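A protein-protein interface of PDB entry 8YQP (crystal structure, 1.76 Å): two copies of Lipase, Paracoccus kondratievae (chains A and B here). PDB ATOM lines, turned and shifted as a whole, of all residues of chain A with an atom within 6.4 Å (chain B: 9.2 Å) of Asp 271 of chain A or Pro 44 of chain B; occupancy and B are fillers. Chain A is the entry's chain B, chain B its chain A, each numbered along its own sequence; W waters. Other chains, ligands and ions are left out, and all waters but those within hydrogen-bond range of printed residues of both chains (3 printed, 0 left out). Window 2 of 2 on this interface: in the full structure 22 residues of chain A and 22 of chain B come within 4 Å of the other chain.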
ATOM      1  N   ASP A   4     -30.232  19.666  13.787  1.00  0.00           N
ATOM      2  CA  ASP A   4     -29.097  18.856  13.354  1.00  0.00           C
ATOM      3  C   ASP A   4     -27.819  19.641  13.640  1.00  0.00           C
ATOM      4  O   ASP A   4     -27.595  20.692  13.032  1.00  0.00           O
ATOM      5  CB  ASP A   4     -29.238  18.505  11.869  1.00  0.00           C
ATOM      6  CG  ASP A   4     -28.122  17.556  11.369  1.00  0.00           C
ATOM      7  OD1 ASP A   4     -26.996  17.635  11.900  1.00  0.00           O
ATOM      8  OD2 ASP A   4     -28.358  16.766  10.422  1.00  0.00           O
ATOM      9  N   GLN A   6     -24.753  19.254  12.811  1.00  0.00           N
ATOM     10  CA  GLN A   6     -23.905  19.492  11.649  1.00  0.00           C
ATOM     11  C   GLN A   6     -24.387  20.696  10.855  1.00  0.00           C
ATOM     12  O   GLN A   6     -23.573  21.494  10.375  1.00  0.00           O
ATOM     13  CB  GLN A   6     -23.885  18.258  10.757  1.00  0.00           C
ATOM     14  CG  GLN A   6     -23.124  17.102  11.347  1.00  0.00           C
ATOM     15  CD  GLN A   6     -23.176  15.897  10.446  1.00  0.00           C
ATOM     16  OE1 GLN A   6     -24.099  15.758   9.638  1.00  0.00           O
ATOM     17  NE2 GLN A   6     -22.220  14.990  10.604  1.00  0.00           N
ATOM     18  N   ALA A 266     -22.849  22.625   1.996  1.00  0.00           N
ATOM     19  CA  ALA A 266     -22.667  21.897   3.235  1.00  0.00           C
ATOM     20  C   ALA A 266     -22.369  20.424   3.010  1.00  0.00           C
ATOM     21  O   ALA A 266     -22.244  19.680   3.990  1.00  0.00           O
ATOM     22  CB  ALA A 266     -23.926  22.029   4.103  1.00  0.00           C
ATOM     23  N   ARG A 267     -22.264  19.983   1.754  1.00  0.00           N
ATOM     24  CA  ARG A 267     -22.160  18.550   1.500  1.00  0.00           C
ATOM     25  C   ARG A 267     -20.878  17.937   2.057  1.00  0.00           C
ATOM     26  O   ARG A 267     -20.823  16.710   2.228  1.00  0.00           O
ATOM     27  CB  ARG A 267     -22.271  18.240   0.004  1.00  0.00           C
ATOM     28  CG  ARG A 267     -21.157  18.801  -0.874  1.00  0.00           C
ATOM     29  CD  ARG A 267     -21.458  18.574  -2.372  1.00  0.00           C
ATOM     30  NE  ARG A 267     -20.297  18.892  -3.202  1.00  0.00           N
ATOM     31  CZ  ARG A 267     -19.783  20.110  -3.342  1.00  0.00           C
ATOM     32  NH1 ARG A 267     -20.390  21.187  -2.842  1.00  0.00           N
ATOM     33  NH2 ARG A 267     -18.632  20.256  -4.002  1.00  0.00           N
ATOM     34  N   GLU A 269     -19.672  18.604   5.130  1.00  0.00           N
ATOM     35  CA  GLU A 269     -19.731  18.562   6.585  1.00  0.00           C
ATOM     36  C   GLU A 269     -21.084  18.128   7.132  1.00  0.00           C
ATOM     37  O   GLU A 269     -21.248  18.118   8.356  1.00  0.00           O
ATOM     38  CB  GLU A 269     -19.377  19.928   7.195  1.00  0.00           C
ATOM     39  CG  GLU A 269     -20.326  21.072   6.794  1.00  0.00           C
ATOM     40  CD  GLU A 269     -19.763  22.458   7.137  1.00  0.00           C
ATOM     41  OE1 GLU A 269     -19.894  22.913   8.304  1.00  0.00           O
ATOM     42  OE2 GLU A 269     -19.146  23.061   6.240  1.00  0.00           O
ATOM     43  N   SER A 270     -22.055  17.794   6.284  1.00  0.00           N
ATOM     44  CA  SER A 270     -23.410  17.450   6.721  1.00  0.00           C
ATOM     45  C   SER A 270     -23.848  16.174   6.026  1.00  0.00           C
ATOM     46  O   SER A 270     -23.895  16.132   4.791  1.00  0.00           O
ATOM     47  CB  SER A 270     -24.406  18.570   6.401  1.00  0.00           C
ATOM     48  OG  SER A 270     -25.755  18.047   6.467  1.00  0.00           O
ATOM     49  N   ASP A 271     -24.203  15.143   6.813  1.00  0.00           N
ATOM     50  CA  ASP A 271     -24.717  13.922   6.201  1.00  0.00           C
ATOM     51  C   ASP A 271     -25.968  14.199   5.380  1.00  0.00           C
ATOM     52  O   ASP A 271     -26.122  13.672   4.277  1.00  0.00           O
ATOM     53  CB  ASP A 271     -25.011  12.872   7.276  1.00  0.00           C
ATOM     54  CG  ASP A 271     -23.754  12.289   7.880  1.00  0.00           C
ATOM     55  OD1 ASP A 271     -22.980  11.593   7.152  1.00  0.00           O
ATOM     56  OD2 ASP A 271     -23.543  12.511   9.083  1.00  0.00           O
ATOM     57  N   ARG A 272     -26.875  15.023   5.902  1.00  0.00           N
ATOM     58  CA  ARG A 272     -28.101  15.339   5.178  1.00  0.00           C
ATOM     59  C   ARG A 272     -27.808  15.968   3.824  1.00  0.00           C
ATOM     60  O   ARG A 272     -28.411  15.596   2.809  1.00  0.00           O
ATOM     61  CB  ARG A 272     -28.962  16.286   6.028  1.00  0.00           C
ATOM     62  CG  ARG A 272     -29.631  15.532   7.188  1.00  0.00           C
ATOM     63  CD  ARG A 272     -30.536  16.487   7.980  1.00  0.00           C
ATOM     64  NE  ARG A 272     -30.811  15.981   9.323  1.00  0.00           N
ATOM     65  CZ  ARG A 272     -31.840  15.208   9.648  1.00  0.00           C
ATOM     66  NH1 ARG A 272     -32.704  14.782   8.742  1.00  0.00           N
ATOM     67  NH2 ARG A 272     -32.027  14.879  10.921  1.00  0.00           N
ATOM     68  N   ALA A 273     -26.913  16.966   3.805  1.00  0.00           N
ATOM     69  CA  ALA A 273     -26.586  17.667   2.570  1.00  0.00           C
ATOM     70  C   ALA A 273     -25.850  16.756   1.605  1.00  0.00           C
ATOM     71  O   ALA A 273     -26.100  16.793   0.398  1.00  0.00           O
ATOM     72  CB  ALA A 273     -25.732  18.898   2.871  1.00  0.00           C
ATOM     73  N   ARG A 274     -24.985  15.897   2.131  1.00  0.00           N
ATOM     74  CA  ARG A 274     -24.249  14.963   1.277  1.00  0.00           C
ATOM     75  C   ARG A 274     -25.203  13.964   0.637  1.00  0.00           C
ATOM     76  O   ARG A 274     -25.119  13.716  -0.568  1.00  0.00           O
ATOM     77  CB  ARG A 274     -23.166  14.268   2.102  1.00  0.00           C
ATOM     78  CG  ARG A 274     -22.421  13.121   1.373  1.00  0.00           C
ATOM     79  CD  ARG A 274     -21.357  12.515   2.277  1.00  0.00           C
ATOM     80  NE  ARG A 274     -21.916  11.884   3.472  1.00  0.00           N
ATOM     81  CZ  ARG A 274     -22.514  10.702   3.484  1.00  0.00           C
ATOM     82  NH1 ARG A 274     -22.596   9.957   2.393  1.00  0.00           N
ATOM     83  NH2 ARG A 274     -23.009  10.238   4.630  1.00  0.00           N
ATOM     84  N   ARG A 275     -26.164  13.423   1.415  1.00  0.00           N
ATOM     85  CA  ARG A 275     -27.136  12.518   0.815  1.00  0.00           C
ATOM     86  C   ARG A 275     -27.957  13.231  -0.248  1.00  0.00           C
ATOM     87  O   ARG A 275     -28.295  12.632  -1.277  1.00  0.00           O
ATOM     88  CB  ARG A 275     -28.051  11.903   1.884  1.00  0.00           C
ATOM     89  CG  ARG A 275     -27.350  10.885   2.788  1.00  0.00           C
ATOM     90  CD  ARG A 275     -28.353  10.051   3.613  1.00  0.00           C
ATOM     91  NE  ARG A 275     -29.383  10.874   4.247  1.00  0.00           N
ATOM     92  CZ  ARG A 275     -29.374  11.282   5.512  1.00  0.00           C
ATOM     93  NH1 ARG A 275     -28.418  10.922   6.355  1.00  0.00           N
ATOM     94  NH2 ARG A 275     -30.355  12.073   5.944  1.00  0.00           N
ATOM     95  N   SER A 276     -28.287  14.511  -0.026  1.00  0.00           N
ATOM     96  CA  SER A 276     -29.077  15.229  -1.017  1.00  0.00           C
ATOM     97  C   SER A 276     -28.327  15.338  -2.342  1.00  0.00           C
ATOM     98  O   SER A 276     -28.897  15.101  -3.416  1.00  0.00           O
ATOM     99  CB  SER A 276     -29.442  16.616  -0.505  1.00  0.00           C
ATOM    100  OG  SER A 276     -30.420  17.160  -1.361  1.00  0.00           O
ATOM    101  N   ALA B  39     -18.959   1.001  14.028  1.00  0.00           N
ATOM    102  CA  ALA B  39     -19.719   1.989  14.777  1.00  0.00           C
ATOM    103  C   ALA B  39     -19.040   3.353  14.758  1.00  0.00           C
ATOM    104  O   ALA B  39     -19.723   4.375  14.839  1.00  0.00           O
ATOM    105  CB  ALA B  39     -19.926   1.528  16.215  1.00  0.00           C
ATOM    106  N   PHE B  41     -17.665   4.841  12.330  1.00  0.00           N
ATOM    107  CA  PHE B  41     -17.839   5.488  11.040  1.00  0.00           C
ATOM    108  C   PHE B  41     -19.276   5.505  10.536  1.00  0.00           C
ATOM    109  O   PHE B  41     -19.587   6.280   9.617  1.00  0.00           O
ATOM    110  CB  PHE B  41     -16.930   4.795  10.022  1.00  0.00           C
ATOM    111  CG  PHE B  41     -15.473   4.923  10.359  1.00  0.00           C
ATOM    112  CD1 PHE B  41     -14.832   6.146  10.243  1.00  0.00           C
ATOM    113  CD2 PHE B  41     -14.754   3.831  10.824  1.00  0.00           C
ATOM    114  CE1 PHE B  41     -13.494   6.289  10.561  1.00  0.00           C
ATOM    115  CE2 PHE B  41     -13.405   3.958  11.144  1.00  0.00           C
ATOM    116  CZ  PHE B  41     -12.774   5.205  11.018  1.00  0.00           C
ATOM    117  N   ARG B  42     -20.155   4.702  11.127  1.00  0.00           N
ATOM    118  CA  ARG B  42     -21.540   4.591  10.686  1.00  0.00           C
ATOM    119  C   ARG B  42     -22.225   5.948  10.644  1.00  0.00           C
ATOM    120  O   ARG B  42     -22.244   6.667  11.645  1.00  0.00           O
ATOM    121  CB  ARG B  42     -22.299   3.690  11.643  1.00  0.00           C
ATOM    122  CG  ARG B  42     -23.695   3.350  11.178  1.00  0.00           C
ATOM    123  CD  ARG B  42     -24.324   2.403  12.187  1.00  0.00           C
ATOM    124  NE  ARG B  42     -23.904   1.051  11.860  1.00  0.00           N
ATOM    125  CZ  ARG B  42     -23.219   0.281  12.695  1.00  0.00           C
ATOM    126  NH1 ARG B  42     -23.003   0.647  13.950  1.00  0.00           N
ATOM    127  NH2 ARG B  42     -22.734  -0.877  12.261  1.00  0.00           N
ATOM    128  N   GLY B  43     -22.803   6.280   9.489  1.00  0.00           N
ATOM    129  CA  GLY B  43     -23.631   7.452   9.345  1.00  0.00           C
ATOM    130  C   GLY B  43     -25.070   7.127   9.689  1.00  0.00           C
ATOM    131  O   GLY B  43     -25.461   5.963   9.824  1.00  0.00           O
ATOM    132  N   PRO B  44     -25.891   8.158   9.825  1.00  0.00           N
ATOM    133  CA  PRO B  44     -27.300   7.949  10.176  1.00  0.00           C
ATOM    134  C   PRO B  44     -28.129   7.453   9.003  1.00  0.00           C
ATOM    135  O   PRO B  44     -27.824   7.687   7.830  1.00  0.00           O
ATOM    136  CB  PRO B  44     -27.762   9.347  10.599  1.00  0.00           C
ATOM    137  CG  PRO B  44     -26.889  10.281   9.807  1.00  0.00           C
ATOM    138  CD  PRO B  44     -25.541   9.582   9.698  1.00  0.00           C
ATOM    139  N   ARG B  45     -29.201   6.751   9.338  1.00  0.00           N
ATOM    140  CA  ARG B  45     -30.151   6.361   8.318  1.00  0.00           C
ATOM    141  C   ARG B  45     -30.943   7.583   7.863  1.00  0.00           C
ATOM    142  O   ARG B  45     -31.215   8.489   8.661  1.00  0.00           O
ATOM    143  CB  ARG B  45     -31.107   5.313   8.867  1.00  0.00           C
ATOM    144  CG  ARG B  45     -30.581   3.930   8.707  1.00  0.00           C
ATOM    145  CD  ARG B  45     -31.712   2.948   8.830  1.00  0.00           C
ATOM    146  NE  ARG B  45     -31.224   1.609   9.086  1.00  0.00           N
ATOM    147  CZ  ARG B  45     -31.943   0.670   9.691  1.00  0.00           C
ATOM    148  NH1 ARG B  45     -33.170   0.911  10.130  1.00  0.00           N
ATOM    149  NH2 ARG B  45     -31.417  -0.538   9.863  1.00  0.00           N
ATOM    150  N   PRO B  46     -31.315   7.644   6.589  1.00  0.00           N
ATOM    151  CA  PRO B  46     -32.303   8.639   6.154  1.00  0.00           C
ATOM    152  C   PRO B  46     -33.599   8.460   6.923  1.00  0.00           C
ATOM    153  O   PRO B  46     -34.147   7.350   6.971  1.00  0.00           O
ATOM    154  CB  PRO B  46     -32.480   8.324   4.658  1.00  0.00           C
ATOM    155  CG  PRO B  46     -31.189   7.634   4.280  1.00  0.00           C
ATOM    156  CD  PRO B  46     -30.837   6.812   5.470  1.00  0.00           C
ATOM    157  N   PRO B  47     -34.089   9.511   7.580  1.00  0.00           N
ATOM    158  CA  PRO B  47     -35.238   9.347   8.496  1.00  0.00           C
ATOM    159  C   PRO B  47     -36.537   8.869   7.850  1.00  0.00           C
ATOM    160  O   PRO B  47     -37.363   8.263   8.551  1.00  0.00           O
ATOM    161  CB  PRO B  47     -35.409  10.757   9.077  1.00  0.00           C
ATOM    162  CG  PRO B  47     -34.033  11.293   9.125  1.00  0.00           C
ATOM    163  CD  PRO B  47     -33.284  10.698   7.927  1.00  0.00           C
ATOM    164  N   GLY B  48     -36.768   9.135   6.566  1.00  0.00           N
ATOM    165  CA  GLY B  48     -38.011   8.718   5.949  1.00  0.00           C
ATOM    166  C   GLY B  48     -37.993   7.354   5.281  1.00  0.00           C
ATOM    167  O   GLY B  48     -39.014   6.921   4.737  1.00  0.00           O
ATOM    168  N   LEU B  49     -36.865   6.654   5.322  1.00  0.00           N
ATOM    169  CA  LEU B  49     -36.674   5.428   4.552  1.00  0.00           C
ATOM    170  C   LEU B  49     -37.216   4.211   5.297  1.00  0.00           C
ATOM    171  O   LEU B  49     -36.853   3.963   6.451  1.00  0.00           O
ATOM    172  CB  LEU B  49     -35.189   5.242   4.251  1.00  0.00           C
ATOM    173  CG  LEU B  49     -34.786   4.072   3.343  1.00  0.00           C
ATOM    174  CD1 LEU B  49     -35.108   4.340   1.880  1.00  0.00           C
ATOM    175  CD2 LEU B  49     -33.311   3.793   3.519  1.00  0.00           C
ATOM    176  N   TYR B  64     -34.353  -2.191   2.043  1.00  0.00           N
ATOM    177  CA  TYR B  64     -34.373  -0.737   2.191  1.00  0.00           C
ATOM    178  C   TYR B  64     -35.202  -0.103   1.077  1.00  0.00           C
ATOM    179  O   TYR B  64     -34.890  -0.270  -0.102  1.00  0.00           O
ATOM    180  CB  TYR B  64     -32.958  -0.144   2.151  1.00  0.00           C
ATOM    181  CG  TYR B  64     -31.928  -0.757   3.079  1.00  0.00           C
ATOM    182  CD1 TYR B  64     -31.343  -1.989   2.802  1.00  0.00           C
ATOM    183  CD2 TYR B  64     -31.520  -0.078   4.216  1.00  0.00           C
ATOM    184  CE1 TYR B  64     -30.404  -2.526   3.649  1.00  0.00           C
ATOM    185  CE2 TYR B  64     -30.590  -0.611   5.070  1.00  0.00           C
ATOM    186  CZ  TYR B  64     -30.029  -1.829   4.781  1.00  0.00           C
ATOM    187  OH  TYR B  64     -29.083  -2.361   5.628  1.00  0.00           O
ATOM    188  N   ASP B  89     -24.886  -1.127   6.877  1.00  0.00           N
ATOM    189  CA  ASP B  89     -26.265  -0.653   6.856  1.00  0.00           C
ATOM    190  C   ASP B  89     -26.375   0.741   6.257  1.00  0.00           C
ATOM    191  O   ASP B  89     -27.281   1.011   5.461  1.00  0.00           O
ATOM    192  CB  ASP B  89     -26.835  -0.650   8.278  1.00  0.00           C
ATOM    193  CG  ASP B  89     -28.298  -0.246   8.316  1.00  0.00           C
ATOM    194  OD1 ASP B  89     -29.156  -1.098   8.005  1.00  0.00           O
ATOM    195  OD2 ASP B  89     -28.588   0.926   8.627  1.00  0.00           O
ATOM    196  N   ASP B  90     -25.470   1.644   6.628  1.00  0.00           N
ATOM    197  CA  ASP B  90     -25.610   3.019   6.157  1.00  0.00           C
ATOM    198  C   ASP B  90     -25.320   3.141   4.663  1.00  0.00           C
ATOM    199  O   ASP B  90     -25.961   3.951   3.985  1.00  0.00           O
ATOM    200  CB  ASP B  90     -24.738   3.962   6.995  1.00  0.00           C
ATOM    201  CG  ASP B  90     -23.265   3.653   6.890  1.00  0.00           C
ATOM    202  OD1 ASP B  90     -22.925   2.492   6.574  1.00  0.00           O
ATOM    203  OD2 ASP B  90     -22.445   4.553   7.189  1.00  0.00           O
ATOM    204  N   VAL B  91     -24.399   2.326   4.126  1.00  0.00           N
ATOM    205  CA  VAL B  91     -24.142   2.308   2.683  1.00  0.00           C
ATOM    206  C   VAL B  91     -25.384   1.881   1.919  1.00  0.00           C
ATOM    207  O   VAL B  91     -25.777   2.515   0.934  1.00  0.00           O
ATOM    208  CB  VAL B  91     -22.954   1.386   2.372  1.00  0.00           C
ATOM    209  CG1 VAL B  91     -22.810   1.196   0.854  1.00  0.00           C
ATOM    210  CG2 VAL B  91     -21.699   1.970   2.966  1.00  0.00           C
ATOM    211  N   CYS B  92     -25.999   0.772   2.347  1.00  0.00           N
ATOM    212  CA  CYS B  92     -27.222   0.294   1.715  1.00  0.00           C
ATOM    213  C   CYS B  92     -28.317   1.345   1.769  1.00  0.00           C
ATOM    214  O   CYS B  92     -29.006   1.600   0.772  1.00  0.00           O
ATOM    215  CB  CYS B  92     -27.686  -0.987   2.404  1.00  0.00           C
ATOM    216  SG  CYS B  92     -26.563  -2.338   1.987  1.00  0.00           S
ATOM    217  N   ALA B  93     -28.504   1.955   2.940  1.00  0.00           N
ATOM    218  CA  ALA B  93     -29.572   2.930   3.089  1.00  0.00           C
ATOM    219  C   ALA B  93     -29.340   4.125   2.175  1.00  0.00           C
ATOM    220  O   ALA B  93     -30.282   4.654   1.573  1.00  0.00           O
ATOM    221  CB  ALA B  93     -29.674   3.357   4.555  1.00  0.00           C
ATOM    222  N   GLU B  94     -28.072   4.524   2.015  1.00  0.00           N
ATOM    223  CA  GLU B  94     -27.742   5.651   1.148  1.00  0.00           C
ATOM    224  C   GLU B  94     -27.919   5.314  -0.320  1.00  0.00           C
ATOM    225  O   GLU B  94     -28.335   6.174  -1.102  1.00  0.00           O
ATOM    226  CB  GLU B  94     -26.313   6.106   1.435  1.00  0.00           C
ATOM    227  CG  GLU B  94     -26.254   6.918   2.725  1.00  0.00           C
ATOM    228  CD  GLU B  94     -24.881   7.482   3.009  1.00  0.00           C
ATOM    229  OE1 GLU B  94     -24.068   7.632   2.060  1.00  0.00           O
ATOM    230  OE2 GLU B  94     -24.631   7.793   4.196  1.00  0.00           O
ATOM    231  N   ASP B  97     -31.721   5.547  -0.769  1.00  0.00           N
ATOM    232  CA  ASP B  97     -32.166   6.940  -0.719  1.00  0.00           C
ATOM    233  C   ASP B  97     -31.794   7.700  -1.991  1.00  0.00           C
ATOM    234  O   ASP B  97     -32.600   8.479  -2.515  1.00  0.00           O
ATOM    235  CB  ASP B  97     -31.541   7.634   0.485  1.00  0.00           C
ATOM    236  CG  ASP B  97     -32.136   9.018   0.743  1.00  0.00           C
ATOM    237  OD1 ASP B  97     -33.365   9.226   0.598  1.00  0.00           O
ATOM    238  OD2 ASP B  97     -31.324   9.933   0.951  1.00  0.00           O
ATOM    239  N   ARG B 265     -16.085   3.611   4.140  1.00  0.00           N
ATOM    240  CA  ARG B 265     -16.287   4.146   5.474  1.00  0.00           C
ATOM    241  C   ARG B 265     -15.695   5.545   5.645  1.00  0.00           C
ATOM    242  O   ARG B 265     -16.029   6.223   6.618  1.00  0.00           O
ATOM    243  CB  ARG B 265     -15.702   3.169   6.494  1.00  0.00           C
ATOM    244  CG  ARG B 265     -16.581   1.885   6.642  1.00  0.00           C
ATOM    245  CD  ARG B 265     -16.008   0.842   7.574  1.00  0.00           C
ATOM    246  NE  ARG B 265     -16.470  -0.513   7.242  1.00  0.00           N
ATOM    247  CZ  ARG B 265     -17.732  -0.900   7.350  1.00  0.00           C
ATOM    248  NH1 ARG B 265     -18.679  -0.063   7.743  1.00  0.00           N
ATOM    249  NH2 ARG B 265     -18.057  -2.159   7.051  1.00  0.00           N
ATOM    250  N   ALA B 266     -14.873   6.011   4.704  1.00  0.00           N
ATOM    251  CA  ALA B 266     -14.281   7.350   4.777  1.00  0.00           C
ATOM    252  C   ALA B 266     -15.092   8.417   4.047  1.00  0.00           C
ATOM    253  O   ALA B 266     -14.673   9.591   4.008  1.00  0.00           O
ATOM    254  CB  ALA B 266     -12.856   7.324   4.197  1.00  0.00           C
ATOM    255  N   ARG B 267     -16.237   8.053   3.464  1.00  0.00           N
ATOM    256  CA  ARG B 267     -16.942   8.979   2.583  1.00  0.00           C
ATOM    257  C   ARG B 267     -17.515  10.172   3.323  1.00  0.00           C
ATOM    258  O   ARG B 267     -17.820  11.190   2.687  1.00  0.00           O
ATOM    259  CB  ARG B 267     -18.048   8.249   1.816  1.00  0.00           C
ATOM    260  CG  ARG B 267     -19.284   7.937   2.656  1.00  0.00           C
ATOM    261  CD  ARG B 267     -20.174   6.898   1.978  1.00  0.00           C
ATOM    262  NE  ARG B 267     -21.349   6.685   2.817  1.00  0.00           N
ATOM    263  CZ  ARG B 267     -21.312   6.029   3.969  1.00  0.00           C
ATOM    264  NH1 ARG B 267     -20.230   5.368   4.352  1.00  0.00           N
ATOM    265  NH2 ARG B 267     -22.381   6.045   4.762  1.00  0.00           N
ATOM    266  N   ARG B 268     -17.635  10.081   4.644  1.00  0.00           N
ATOM    267  CA  ARG B 268     -18.122  11.174   5.485  1.00  0.00           C
ATOM    268  C   ARG B 268     -17.019  12.124   5.923  1.00  0.00           C
ATOM    269  O   ARG B 268     -17.312  13.133   6.568  1.00  0.00           O
ATOM    270  CB  ARG B 268     -18.807  10.605   6.724  1.00  0.00           C
ATOM    271  CG  ARG B 268     -19.929   9.658   6.417  1.00  0.00           C
ATOM    272  CD  ARG B 268     -20.449   9.004   7.691  1.00  0.00           C
ATOM    273  NE  ARG B 268     -21.139   9.958   8.559  1.00  0.00           N
ATOM    274  CZ  ARG B 268     -20.979  10.026   9.873  1.00  0.00           C
ATOM    275  NH1 ARG B 268     -20.135   9.231  10.505  1.00  0.00           N
ATOM    276  NH2 ARG B 268     -21.699  10.906  10.576  1.00  0.00           N
ATOM    277  N   GLU B 269     -15.761  11.829   5.609  1.00  0.00           N
ATOM    278  CA  GLU B 269     -14.660  12.671   6.050  1.00  0.00           C
ATOM    279  C   GLU B 269     -13.555  12.856   5.011  1.00  0.00           C
ATOM    280  O   GLU B 269     -12.583  13.573   5.289  1.00  0.00           O
ATOM    281  CB  GLU B 269     -14.087  12.100   7.360  1.00  0.00           C
ATOM    282  CG  GLU B 269     -13.178  10.887   7.204  1.00  0.00           C
ATOM    283  CD  GLU B 269     -12.847  10.276   8.546  1.00  0.00           C
ATOM    284  OE1 GLU B 269     -13.676   9.485   9.040  1.00  0.00           O
ATOM    285  OE2 GLU B 269     -11.777  10.597   9.115  1.00  0.00           O
ATOM    286  N   ARG B 274     -15.620  10.434  -0.731  1.00  0.00           N
ATOM    287  CA  ARG B 274     -16.958  10.937  -1.015  1.00  0.00           C
ATOM    288  C   ARG B 274     -17.226  10.983  -2.520  1.00  0.00           C
ATOM    289  O   ARG B 274     -18.295  10.569  -2.979  1.00  0.00           O
ATOM    290  CB  ARG B 274     -17.135  12.323  -0.371  1.00  0.00           C
ATOM    291  CG  ARG B 274     -18.524  12.865  -0.540  1.00  0.00           C
ATOM    292  CD  ARG B 274     -18.726  14.303   0.022  1.00  0.00           C
ATOM    293  NE  ARG B 274     -17.667  15.223  -0.377  1.00  0.00           N
ATOM    294  CZ  ARG B 274     -17.714  15.901  -1.510  1.00  0.00           C
ATOM    295  NH1 ARG B 274     -18.705  15.719  -2.366  1.00  0.00           N
ATOM    296  NH2 ARG B 274     -16.730  16.755  -1.806  1.00  0.00           N
HETATM  297  O   HOH W   1     -26.305   9.023   6.284  1.00  0.00           O
HETATM  298  O   HOH W   2     -29.813  10.329  -1.084  1.00  0.00           O
HETATM  299  O   HOH W   3     -31.769  11.977   3.147  1.00  0.00           O
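Among the printed residues, merely in contact across the chains: Arg 274 of chain A with Arg 267 of chain B (3.5 Å), Asp 271 of chain A with Pro 44 of chain B (3.6 Å), Arg 275 of chain A with Pro 44 of chain B (3.6 Å), Arg 274 of chain A with Arg 268 of chain B (3.6 Å), Arg 267 of chain A with Arg 274 of chain B (3.6 Å), Arg 275 of chain A with Pro 46 of chain B (3.7 Å), Arg 272 of chain A with Pro 47 of chain B (3.8 Å), Arg 275 of chain A with Pro 47 of chain B (3.8 Å), Arg 275 of chain A with Glu 94 of chain B (3.9 Å) and Arg 274 of chain A with Arg 274 of chain B (3.9 Å).
NH2 of Arg 274 of chain A is in salt-bridge range of OD1 of Asp 271 of chain A (2.9 Å).
The guanidinium group (NE) of Arg 272 of chain A is in salt-bridge range of the side-chain carboxylate (OD2) of Asp 4 of chain A (2.8 Å).
The backbone NH of Asp 271 of chain A lies within hydrogen-bond range of the side-chain amide oxygen of Gln 6 of chain A (2.9 Å).
The side-chain hydroxyl (OG) of Ser 270 of chain A lies close to the backbone NH (N) of Arg 272 of chain A, at 3.3 Å.
The backbone carbonyl oxygen of Phe 41 of chain B lies within hydrogen-bond range of the guanidinium group of Arg 268 of chain B, at 3.1 Å.
The side-chain carboxylate of Asp 90 of chain B is in salt-bridge range of the guanidinium group of Arg 267 of chain B (2.8 Å).
Asp 4 of chain A touches none of the printed residues of chain B.
Printed residues of chain B within 4 Å of Arg 267 of chain A: Arg 274.
No residue of chain B comes within 4 Å of Ser 270 of chain A.
Of chain B, only Pro 44 (3.6 Å) and Arg 268 (2.8 Å) come within 4 Å of Asp 271 of chain A.
Of the printed residues of chain B, Arg 274 of chain A touches Glu 94 (2.8 Å), Arg 267 (3.5 Å), Arg 268 (3.6 Å) and Arg 274 (3.9 Å).
Pro 44 of chain B touches just these residues of chain A: Asp 271 and Arg 275.
Printed residues of chain A within 4 Å of Pro 47 of chain B: Arg 272 and Arg 275.
Of the printed residues of chain A, Arg 267 of chain B touches Arg 274.
Of the printed residues of chain A, Arg 268 of chain B touches Asp 271 (2.8 Å) and Arg 274 (3.6 Å).
Glu 269 of chain B touches none of the printed residues of chain A.
The nearest residue of chain A that does not touch Pro 44 of chain B is Arg 274 of chain A (5.7 Å).
Printed residues of chain B that touch a printed residue of chain A: Pro 44, Pro 46, Pro 47, Glu 94, Asp 97, Arg 267, Arg 268 and Arg 274.
Among the printed residues, 13 pairs touch across the chains.
Among the printed residues, Asp or Glu carboxylates within 4 Å of a Lys or Arg side-chain nitrogen of the other chain: Asp 271 of chain A with Arg 268 of chain B (2.8 Å), Arg 274 of chain A with Glu 94 of chain B (2.8 Å) and Arg 275 of chain A with Asp 97 of chain B (3.9 Å).
OD1 of Asp 271 of chain A is in salt-bridge range of NE of Arg 268 of chain B (2.8 Å).
NE of Arg 275 of chain A is in salt-bridge range of OD2 of Asp 97 of chain B (3.9 Å).
NH1 of Arg 274 of chain A is in salt-bridge range of OE1 of Glu 94 of chain B.
Water W1 lies within hydrogen-bond range of O of Pro 44 of chain B (2.5 Å), NH1 of Arg 275 of chain A (2.8 Å) and OE2 of Glu 94 of chain B (2.9 Å).
Water W2 bridges the side-chain carboxylate (OD2) of Asp 97 of chain B (2.6 Å) and the backbone carbonyl oxygen (O) of Arg 275 of chain A (2.8 Å).
Water W3 bridges NE of Arg 275 of chain A (2.8 Å) and OD2 of Asp 97 of chain B (3.0 Å).
Arg 267 of chain A touches Arg 274 of chain B, and with the chains exchanged Arg 274 of chain A touches Arg 267 of chain B.
Arg 274 of chain A touches its own counterpart, Arg 274 of chain B.
4 positions are printed for both chains.
Of the 13 pairs that touch across the chains among the printed residues, 3 have their exchanged pair printed and touching as well.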
